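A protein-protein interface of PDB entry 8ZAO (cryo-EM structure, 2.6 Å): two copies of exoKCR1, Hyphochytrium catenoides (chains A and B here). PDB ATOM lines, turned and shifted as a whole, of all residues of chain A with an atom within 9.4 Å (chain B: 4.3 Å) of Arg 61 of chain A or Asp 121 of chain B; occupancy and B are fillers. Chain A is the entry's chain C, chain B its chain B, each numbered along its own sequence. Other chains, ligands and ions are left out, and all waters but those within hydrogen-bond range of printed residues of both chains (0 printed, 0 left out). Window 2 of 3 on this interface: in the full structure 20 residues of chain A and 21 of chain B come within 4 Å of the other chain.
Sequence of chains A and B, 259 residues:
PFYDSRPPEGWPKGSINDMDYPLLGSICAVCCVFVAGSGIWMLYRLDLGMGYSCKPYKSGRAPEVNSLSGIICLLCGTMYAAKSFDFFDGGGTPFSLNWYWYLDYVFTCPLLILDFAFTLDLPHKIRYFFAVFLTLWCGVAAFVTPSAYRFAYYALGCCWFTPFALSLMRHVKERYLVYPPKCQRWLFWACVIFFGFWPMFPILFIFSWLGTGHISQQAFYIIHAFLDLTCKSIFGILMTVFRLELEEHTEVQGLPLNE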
ATOM      1  N   LEU A  46       1.628  -9.664 -36.670  1.00  0.00           N
ATOM      2  CA  LEU A  46       0.776  -9.454 -35.507  1.00  0.00           C
ATOM      3  C   LEU A  46       0.743 -10.692 -34.623  1.00  0.00           C
ATOM      4  O   LEU A  46       0.796 -10.588 -33.392  1.00  0.00           O
ATOM      5  CB  LEU A  46      -0.632  -9.072 -35.956  1.00  0.00           C
ATOM      6  CG  LEU A  46      -1.645  -8.889 -34.833  1.00  0.00           C
ATOM      7  CD1 LEU A  46      -1.331  -7.632 -34.045  1.00  0.00           C
ATOM      8  CD2 LEU A  46      -3.051  -8.843 -35.389  1.00  0.00           C
ATOM      9  N   ASP A  47       0.661 -11.875 -35.231  1.00  0.00           N
ATOM     10  CA  ASP A  47       0.699 -13.116 -34.469  1.00  0.00           C
ATOM     11  C   ASP A  47       2.071 -13.406 -33.876  1.00  0.00           C
ATOM     12  O   ASP A  47       2.167 -14.224 -32.956  1.00  0.00           O
ATOM     13  CB  ASP A  47       0.263 -14.290 -35.346  1.00  0.00           C
ATOM     14  CG  ASP A  47      -1.126 -14.105 -35.917  1.00  0.00           C
ATOM     15  OD1 ASP A  47      -1.935 -13.383 -35.296  1.00  0.00           O
ATOM     16  OD2 ASP A  47      -1.412 -14.685 -36.985  1.00  0.00           O
ATOM     17  N   LEU A  48       3.129 -12.768 -34.384  1.00  0.00           N
ATOM     18  CA  LEU A  48       4.460 -12.983 -33.824  1.00  0.00           C
ATOM     19  C   LEU A  48       4.552 -12.516 -32.377  1.00  0.00           C
ATOM     20  O   LEU A  48       5.159 -13.199 -31.545  1.00  0.00           O
ATOM     21  CB  LEU A  48       5.511 -12.272 -34.674  1.00  0.00           C
ATOM     22  CG  LEU A  48       6.049 -13.032 -35.889  1.00  0.00           C
ATOM     23  CD1 LEU A  48       7.344 -12.407 -36.373  1.00  0.00           C
ATOM     24  CD2 LEU A  48       6.252 -14.501 -35.563  1.00  0.00           C
ATOM     25  N   GLY A  49       3.967 -11.365 -32.057  1.00  0.00           N
ATOM     26  CA  GLY A  49       4.021 -10.840 -30.706  1.00  0.00           C
ATOM     27  C   GLY A  49       3.932  -9.330 -30.654  1.00  0.00           C
ATOM     28  O   GLY A  49       3.793  -8.677 -31.691  1.00  0.00           O
ATOM     29  N   MET A  50       4.010  -8.762 -29.452  1.00  0.00           N
ATOM     30  CA  MET A  50       3.917  -7.319 -29.270  1.00  0.00           C
ATOM     31  C   MET A  50       5.284  -6.673 -29.457  1.00  0.00           C
ATOM     32  O   MET A  50       6.274  -7.119 -28.871  1.00  0.00           O
ATOM     33  CB  MET A  50       3.366  -6.978 -27.885  1.00  0.00           C
ATOM     34  CG  MET A  50       2.193  -7.831 -27.451  1.00  0.00           C
ATOM     35  SD  MET A  50       1.656  -7.481 -25.767  1.00  0.00           S
ATOM     36  CE  MET A  50       2.992  -8.209 -24.827  1.00  0.00           C
ATOM     37  N   LYS A  55       7.229  -9.709 -27.928  1.00  0.00           N
ATOM     38  CA  LYS A  55       6.825 -10.130 -26.594  1.00  0.00           C
ATOM     39  C   LYS A  55       5.525 -10.921 -26.684  1.00  0.00           C
ATOM     40  O   LYS A  55       4.545 -10.429 -27.256  1.00  0.00           O
ATOM     41  CB  LYS A  55       6.653  -8.917 -25.684  1.00  0.00           C
ATOM     42  CG  LYS A  55       6.531  -9.257 -24.208  1.00  0.00           C
ATOM     43  CD  LYS A  55       6.368  -8.002 -23.369  1.00  0.00           C
ATOM     44  CE  LYS A  55       5.753  -8.319 -22.017  1.00  0.00           C
ATOM     45  NZ  LYS A  55       4.878  -7.216 -21.532  1.00  0.00           N
ATOM     46  N   PRO A  56       5.478 -12.142 -26.152  1.00  0.00           N
ATOM     47  CA  PRO A  56       4.265 -12.959 -26.284  1.00  0.00           C
ATOM     48  C   PRO A  56       3.067 -12.305 -25.614  1.00  0.00           C
ATOM     49  O   PRO A  56       3.187 -11.663 -24.569  1.00  0.00           O
ATOM     50  CB  PRO A  56       4.645 -14.276 -25.597  1.00  0.00           C
ATOM     51  CG  PRO A  56       5.820 -13.944 -24.737  1.00  0.00           C
ATOM     52  CD  PRO A  56       6.552 -12.851 -25.440  1.00  0.00           C
ATOM     53  N   TYR A  57       1.903 -12.474 -26.233  1.00  0.00           N
ATOM     54  CA  TYR A  57       0.668 -11.956 -25.664  1.00  0.00           C
ATOM     55  C   TYR A  57       0.324 -12.700 -24.382  1.00  0.00           C
ATOM     56  O   TYR A  57       0.532 -13.913 -24.274  1.00  0.00           O
ATOM     57  CB  TYR A  57      -0.475 -12.085 -26.669  1.00  0.00           C
ATOM     58  CG  TYR A  57      -0.294 -11.257 -27.919  1.00  0.00           C
ATOM     59  CD1 TYR A  57      -0.685  -9.926 -27.957  1.00  0.00           C
ATOM     60  CD2 TYR A  57       0.264 -11.808 -29.063  1.00  0.00           C
ATOM     61  CE1 TYR A  57      -0.524  -9.169 -29.100  1.00  0.00           C
ATOM     62  CE2 TYR A  57       0.429 -11.058 -30.210  1.00  0.00           C
ATOM     63  CZ  TYR A  57       0.035  -9.739 -30.221  1.00  0.00           C
ATOM     64  OH  TYR A  57       0.200  -8.988 -31.361  1.00  0.00           O
ATOM     65  N   LYS A  58      -0.202 -11.965 -23.401  1.00  0.00           N
ATOM     66  CA  LYS A  58      -0.570 -12.585 -22.132  1.00  0.00           C
ATOM     67  C   LYS A  58      -1.703 -13.586 -22.314  1.00  0.00           C
ATOM     68  O   LYS A  58      -1.698 -14.657 -21.696  1.00  0.00           O
ATOM     69  CB  LYS A  58      -0.951 -11.510 -21.114  1.00  0.00           C
ATOM     70  CG  LYS A  58      -0.311 -11.697 -19.745  1.00  0.00           C
ATOM     71  CD  LYS A  58       1.211 -11.762 -19.826  1.00  0.00           C
ATOM     72  CE  LYS A  58       1.800 -10.552 -20.547  1.00  0.00           C
ATOM     73  NZ  LYS A  58       3.256 -10.718 -20.810  1.00  0.00           N
ATOM     74  N   SER A  59      -2.682 -13.257 -23.156  1.00  0.00           N
ATOM     75  CA  SER A  59      -3.761 -14.182 -23.467  1.00  0.00           C
ATOM     76  C   SER A  59      -3.363 -15.228 -24.499  1.00  0.00           C
ATOM     77  O   SER A  59      -4.148 -16.145 -24.761  1.00  0.00           O
ATOM     78  CB  SER A  59      -4.987 -13.415 -23.966  1.00  0.00           C
ATOM     79  OG  SER A  59      -4.611 -12.371 -24.845  1.00  0.00           O
ATOM     80  N   GLY A  60      -2.174 -15.113 -25.086  1.00  0.00           N
ATOM     81  CA  GLY A  60      -1.735 -16.022 -26.120  1.00  0.00           C
ATOM     82  C   GLY A  60      -2.227 -15.688 -27.509  1.00  0.00           C
ATOM     83  O   GLY A  60      -1.867 -16.389 -28.462  1.00  0.00           O
ATOM     84  N   ARG A  61      -3.035 -14.641 -27.655  1.00  0.00           N
ATOM     85  CA  ARG A  61      -3.578 -14.244 -28.942  1.00  0.00           C
ATOM     86  C   ARG A  61      -3.584 -12.726 -29.033  1.00  0.00           C
ATOM     87  O   ARG A  61      -3.700 -12.028 -28.024  1.00  0.00           O
ATOM     88  CB  ARG A  61      -4.997 -14.789 -29.145  1.00  0.00           C
ATOM     89  CG  ARG A  61      -5.927 -14.511 -27.979  1.00  0.00           C
ATOM     90  CD  ARG A  61      -7.252 -15.231 -28.136  1.00  0.00           C
ATOM     91  NE  ARG A  61      -7.133 -16.658 -27.860  1.00  0.00           N
ATOM     92  CZ  ARG A  61      -8.162 -17.474 -27.693  1.00  0.00           C
ATOM     93  NH1 ARG A  61      -9.408 -17.036 -27.760  1.00  0.00           N
ATOM     94  NH2 ARG A  61      -7.937 -18.762 -27.450  1.00  0.00           N
ATOM     95  N   ALA A  62      -3.456 -12.226 -30.254  1.00  0.00           N
ATOM     96  CA  ALA A  62      -3.479 -10.796 -30.494  1.00  0.00           C
ATOM     97  C   ALA A  62      -4.893 -10.250 -30.336  1.00  0.00           C
ATOM     98  O   ALA A  62      -5.871 -10.993 -30.445  1.00  0.00           O
ATOM     99  CB  ALA A  62      -2.954 -10.494 -31.893  1.00  0.00           C
ATOM    100  N   PRO A  63      -5.028  -8.954 -30.057  1.00  0.00           N
ATOM    101  CA  PRO A  63      -6.363  -8.346 -30.045  1.00  0.00           C
ATOM    102  C   PRO A  63      -7.041  -8.501 -31.398  1.00  0.00           C
ATOM    103  O   PRO A  63      -6.397  -8.431 -32.447  1.00  0.00           O
ATOM    104  CB  PRO A  63      -6.082  -6.877 -29.716  1.00  0.00           C
ATOM    105  CG  PRO A  63      -4.796  -6.907 -28.970  1.00  0.00           C
ATOM    106  CD  PRO A  63      -3.994  -8.017 -29.582  1.00  0.00           C
ATOM    107  N   GLU A  64      -8.356  -8.725 -31.364  1.00  0.00           N
ATOM    108  CA  GLU A  64      -9.088  -8.997 -32.595  1.00  0.00           C
ATOM    109  C   GLU A  64      -9.100  -7.795 -33.529  1.00  0.00           C
ATOM    110  O   GLU A  64      -8.978  -7.960 -34.748  1.00  0.00           O
ATOM    111  CB  GLU A  64     -10.515  -9.433 -32.269  1.00  0.00           C
ATOM    112  CG  GLU A  64     -10.584 -10.623 -31.335  1.00  0.00           C
ATOM    113  CD  GLU A  64     -10.856 -11.919 -32.067  1.00  0.00           C
ATOM    114  OE1 GLU A  64     -11.115 -11.871 -33.287  1.00  0.00           O
ATOM    115  OE2 GLU A  64     -10.806 -12.987 -31.421  1.00  0.00           O
ATOM    116  N   VAL A  65      -9.246  -6.582 -32.985  1.00  0.00           N
ATOM    117  CA  VAL A  65      -9.237  -5.377 -33.808  1.00  0.00           C
ATOM    118  C   VAL A  65      -7.878  -5.109 -34.429  1.00  0.00           C
ATOM    119  O   VAL A  65      -7.799  -4.418 -35.453  1.00  0.00           O
ATOM    120  CB  VAL A  65      -9.678  -4.146 -32.991  1.00  0.00           C
ATOM    121  CG1 VAL A  65     -11.188  -4.119 -32.850  1.00  0.00           C
ATOM    122  CG2 VAL A  65      -9.007  -4.147 -31.628  1.00  0.00           C
ATOM    123  N   ASN A  66      -6.801  -5.634 -33.845  1.00  0.00           N
ATOM    124  CA  ASN A  66      -5.462  -5.457 -34.385  1.00  0.00           C
ATOM    125  C   ASN A  66      -5.268  -6.154 -35.722  1.00  0.00           C
ATOM    126  O   ASN A  66      -4.390  -5.750 -36.493  1.00  0.00           O
ATOM    127  CB  ASN A  66      -4.421  -5.975 -33.390  1.00  0.00           C
ATOM    128  CG  ASN A  66      -4.028  -4.934 -32.366  1.00  0.00           C
ATOM    129  OD1 ASN A  66      -4.754  -3.969 -32.135  1.00  0.00           O
ATOM    130  ND2 ASN A  66      -2.871  -5.125 -31.745  1.00  0.00           N
ATOM    131  N   SER A  67      -6.061  -7.180 -36.015  1.00  0.00           N
ATOM    132  CA  SER A  67      -5.980  -7.895 -37.278  1.00  0.00           C
ATOM    133  C   SER A  67      -6.817  -7.256 -38.374  1.00  0.00           C
ATOM    134  O   SER A  67      -6.982  -7.861 -39.438  1.00  0.00           O
ATOM    135  CB  SER A  67      -6.413  -9.350 -37.086  1.00  0.00           C
ATOM    136  OG  SER A  67      -7.781  -9.518 -37.402  1.00  0.00           O
ATOM    137  N   GLU A 247       3.740  -0.767 -29.145  1.00  0.00           N
ATOM    138  CA  GLU A 247       3.832  -1.890 -28.221  1.00  0.00           C
ATOM    139  C   GLU A 247       5.228  -2.014 -27.629  1.00  0.00           C
ATOM    140  O   GLU A 247       5.372  -2.397 -26.462  1.00  0.00           O
ATOM    141  CB  GLU A 247       3.434  -3.184 -28.928  1.00  0.00           C
ATOM    142  CG  GLU A 247       1.939  -3.336 -29.141  1.00  0.00           C
ATOM    143  CD  GLU A 247       1.602  -4.368 -30.200  1.00  0.00           C
ATOM    144  OE1 GLU A 247       2.445  -4.606 -31.090  1.00  0.00           O
ATOM    145  OE2 GLU A 247       0.495  -4.940 -30.142  1.00  0.00           O
ATOM    146  N   ALA B 117     -16.644 -20.108 -33.130  1.00  0.00           N
ATOM    147  CA  ALA B 117     -15.503 -19.499 -32.457  1.00  0.00           C
ATOM    148  C   ALA B 117     -15.872 -18.984 -31.074  1.00  0.00           C
ATOM    149  O   ALA B 117     -15.090 -19.142 -30.130  1.00  0.00           O
ATOM    150  CB  ALA B 117     -14.935 -18.368 -33.312  1.00  0.00           C
ATOM    151  N   PHE B 118     -17.043 -18.363 -30.933  1.00  0.00           N
ATOM    152  CA  PHE B 118     -17.465 -17.855 -29.633  1.00  0.00           C
ATOM    153  C   PHE B 118     -17.712 -18.977 -28.633  1.00  0.00           C
ATOM    154  O   PHE B 118     -17.348 -18.845 -27.460  1.00  0.00           O
ATOM    155  CB  PHE B 118     -18.722 -16.999 -29.786  1.00  0.00           C
ATOM    156  CG  PHE B 118     -18.436 -15.559 -30.097  1.00  0.00           C
ATOM    157  CD1 PHE B 118     -17.673 -14.791 -29.237  1.00  0.00           C
ATOM    158  CD2 PHE B 118     -18.931 -14.974 -31.248  1.00  0.00           C
ATOM    159  CE1 PHE B 118     -17.406 -13.468 -29.520  1.00  0.00           C
ATOM    160  CE2 PHE B 118     -18.668 -13.651 -31.537  1.00  0.00           C
ATOM    161  CZ  PHE B 118     -17.905 -12.897 -30.671  1.00  0.00           C
ATOM    162  N   THR B 119     -18.329 -20.077 -29.070  1.00  0.00           N
ATOM    163  CA  THR B 119     -18.569 -21.204 -28.179  1.00  0.00           C
ATOM    164  C   THR B 119     -17.273 -21.852 -27.706  1.00  0.00           C
ATOM    165  O   THR B 119     -17.159 -22.212 -26.529  1.00  0.00           O
ATOM    166  CB  THR B 119     -19.444 -22.250 -28.872  1.00  0.00           C
ATOM    167  OG1 THR B 119     -20.533 -21.598 -29.536  1.00  0.00           O
ATOM    168  CG2 THR B 119     -19.995 -23.238 -27.862  1.00  0.00           C
ATOM    169  N   LEU B 120     -16.295 -22.005 -28.596  1.00  0.00           N
ATOM    170  CA  LEU B 120     -15.043 -22.679 -28.280  1.00  0.00           C
ATOM    171  C   LEU B 120     -13.929 -21.713 -27.895  1.00  0.00           C
ATOM    172  O   LEU B 120     -12.803 -22.154 -27.647  1.00  0.00           O
ATOM    173  CB  LEU B 120     -14.598 -23.540 -29.463  1.00  0.00           C
ATOM    174  CG  LEU B 120     -14.917 -25.034 -29.380  1.00  0.00           C
ATOM    175  CD1 LEU B 120     -16.415 -25.266 -29.422  1.00  0.00           C
ATOM    176  CD2 LEU B 120     -14.228 -25.780 -30.506  1.00  0.00           C
ATOM    177  N   ASP B 121     -14.218 -20.414 -27.831  1.00  0.00           N
ATOM    178  CA  ASP B 121     -13.226 -19.383 -27.530  1.00  0.00           C
ATOM    179  C   ASP B 121     -12.029 -19.486 -28.475  1.00  0.00           C
ATOM    180  O   ASP B 121     -10.867 -19.391 -28.077  1.00  0.00           O
ATOM    181  CB  ASP B 121     -12.785 -19.457 -26.065  1.00  0.00           C
ATOM    182  CG  ASP B 121     -12.103 -18.185 -25.596  1.00  0.00           C
ATOM    183  OD1 ASP B 121     -12.486 -17.094 -26.067  1.00  0.00           O
ATOM    184  OD2 ASP B 121     -11.182 -18.275 -24.757  1.00  0.00           O
ATOM    185  N   LEU B 122     -12.340 -19.697 -29.751  1.00  0.00           N
ATOM    186  CA  LEU B 122     -11.296 -19.816 -30.759  1.00  0.00           C
ATOM    187  C   LEU B 122     -10.675 -18.452 -31.048  1.00  0.00           C
ATOM    188  O   LEU B 122     -11.379 -17.439 -31.059  1.00  0.00           O
ATOM    189  CB  LEU B 122     -11.855 -20.405 -32.048  1.00  0.00           C
ATOM    190  CG  LEU B 122     -12.275 -21.873 -31.969  1.00  0.00           C
ATOM    191  CD1 LEU B 122     -13.077 -22.267 -33.193  1.00  0.00           C
ATOM    192  CD2 LEU B 122     -11.059 -22.764 -31.812  1.00  0.00           C
ATOM    193  N   PRO B 123      -9.365 -18.404 -31.276  1.00  0.00           N
ATOM    194  CA  PRO B 123      -8.718 -17.129 -31.591  1.00  0.00           C
ATOM    195  C   PRO B 123      -9.052 -16.666 -33.000  1.00  0.00           C
ATOM    196  O   PRO B 123      -9.481 -17.443 -33.857  1.00  0.00           O
ATOM    197  CB  PRO B 123      -7.226 -17.446 -31.453  1.00  0.00           C
ATOM    198  CG  PRO B 123      -7.134 -18.904 -31.729  1.00  0.00           C
ATOM    199  CD  PRO B 123      -8.399 -19.513 -31.197  1.00  0.00           C
ATOM    200  N   LYS B 125     -11.427 -14.555 -34.303  1.00  0.00           N
ATOM    201  CA  LYS B 125     -12.815 -14.709 -34.726  1.00  0.00           C
ATOM    202  C   LYS B 125     -13.108 -13.878 -35.968  1.00  0.00           C
ATOM    203  O   LYS B 125     -13.800 -14.340 -36.884  1.00  0.00           O
ATOM    204  CB  LYS B 125     -13.749 -14.324 -33.581  1.00  0.00           C
ATOM    205  CG  LYS B 125     -13.450 -15.053 -32.284  1.00  0.00           C
ATOM    206  CD  LYS B 125     -14.531 -14.819 -31.248  1.00  0.00           C
ATOM    207  CE  LYS B 125     -14.258 -15.616 -29.985  1.00  0.00           C
ATOM    208  NZ  LYS B 125     -12.803 -15.757 -29.721  1.00  0.00           N
ATOM    209  N   ARG B 175      -8.433 -26.616 -28.473  1.00  0.00           N
ATOM    210  CA  ARG B 175      -9.544 -26.501 -27.540  1.00  0.00           C
ATOM    211  C   ARG B 175     -10.092 -27.864 -27.140  1.00  0.00           C
ATOM    212  O   ARG B 175     -10.640 -28.006 -26.042  1.00  0.00           O
ATOM    213  CB  ARG B 175     -10.655 -25.645 -28.145  1.00  0.00           C
ATOM    214  CG  ARG B 175     -10.301 -24.173 -28.263  1.00  0.00           C
ATOM    215  CD  ARG B 175      -9.816 -23.614 -26.937  1.00  0.00           C
ATOM    216  NE  ARG B 175     -10.915 -23.273 -26.044  1.00  0.00           N
ATOM    217  CZ  ARG B 175     -10.759 -22.843 -24.800  1.00  0.00           C
ATOM    218  NH1 ARG B 175      -9.559 -22.698 -24.265  1.00  0.00           N
ATOM    219  NH2 ARG B 175     -11.834 -22.552 -24.075  1.00  0.00           N
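The side-chain amino group (NZ) of Lys 125 of chain B lies within salt-bridge range of the side-chain carboxylate (OE2) of Glu 64 of chain A (3.8 Å). OD1 of Asp 121 of chain B is in salt-bridge range of NH1 of Arg 61 of chain A, 3.5 Å away.
Hydrophobic or aromatic side chains of chain B within 4 Å of the printed part of chain A: Pro 123. Among the printed residues, Asp or Glu carboxylates within 4 Å of a Lys or Arg side-chain nitrogen of the other chain: Arg 61 of chain A with Asp 121 of chain B (3.5 Å) and Glu 64 of chain A with Lys 125 of chain B (3.8 Å).
No position is printed for both chains. Of the 4 pairs that touch across the chains among the printed residues, none has its exchanged pair printed and touching as well.
Of the printed residues of chain B, Arg 61 of chain A touches Asp 121, Leu 122 and Pro 123. Asp 121 of chain B touches just one residue of chain A: Arg 61 (2.8 Å). Of the printed residues of chain A, Lys 125 of chain B touches Glu 64 (2.9 Å). Of the printed residues of chain B, Glu 64 of chain A touches Lys 125 (2.9 Å). Of the printed residues of chain A, Pro 123 of chain B touches Arg 61 (3.7 Å). Printed residues of chain A within 4 Å of Leu 122 of chain B: Arg 61 (3.8 Å). The nearest residue of chain B that does not touch Arg 61 of chain A is Lys 125 of chain B (4.1 Å). The nearest residue of chain A that does not touch Asp 121 of chain B is Glu 64 of chain A (7.0 Å). The nearest printed residue of chain A that does not touch Lys 125 of chain B is Arg 61 of chain A (4.1 Å).
Arg 61 of chain A touches Leu 122 of chain B. Pro 123 of chain B touches Arg 61 of chain A.
The backbone carbonyl oxygen (O) of Arg 61 of chain A sits at hydrogen-bond distance from the side-chain hydroxyl (OG) of Ser 59 of chain A (3.3 Å). The side-chain hydroxyl (OG) of Ser 67 of chain A lies within hydrogen-bond range of the backbone carbonyl oxygen (O) of Glu 64 of chain A. O of Leu 122 of chain B sits at hydrogen-bond distance from NZ of Lys 125 of chain B. NZ of Lys 125 of chain B is in salt-bridge range of OD1 of Asp 121 of chain B (3.9 Å). N of Leu 122 of chain B lies within hydrogen-bond range of O of Ala 117 of chain B.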
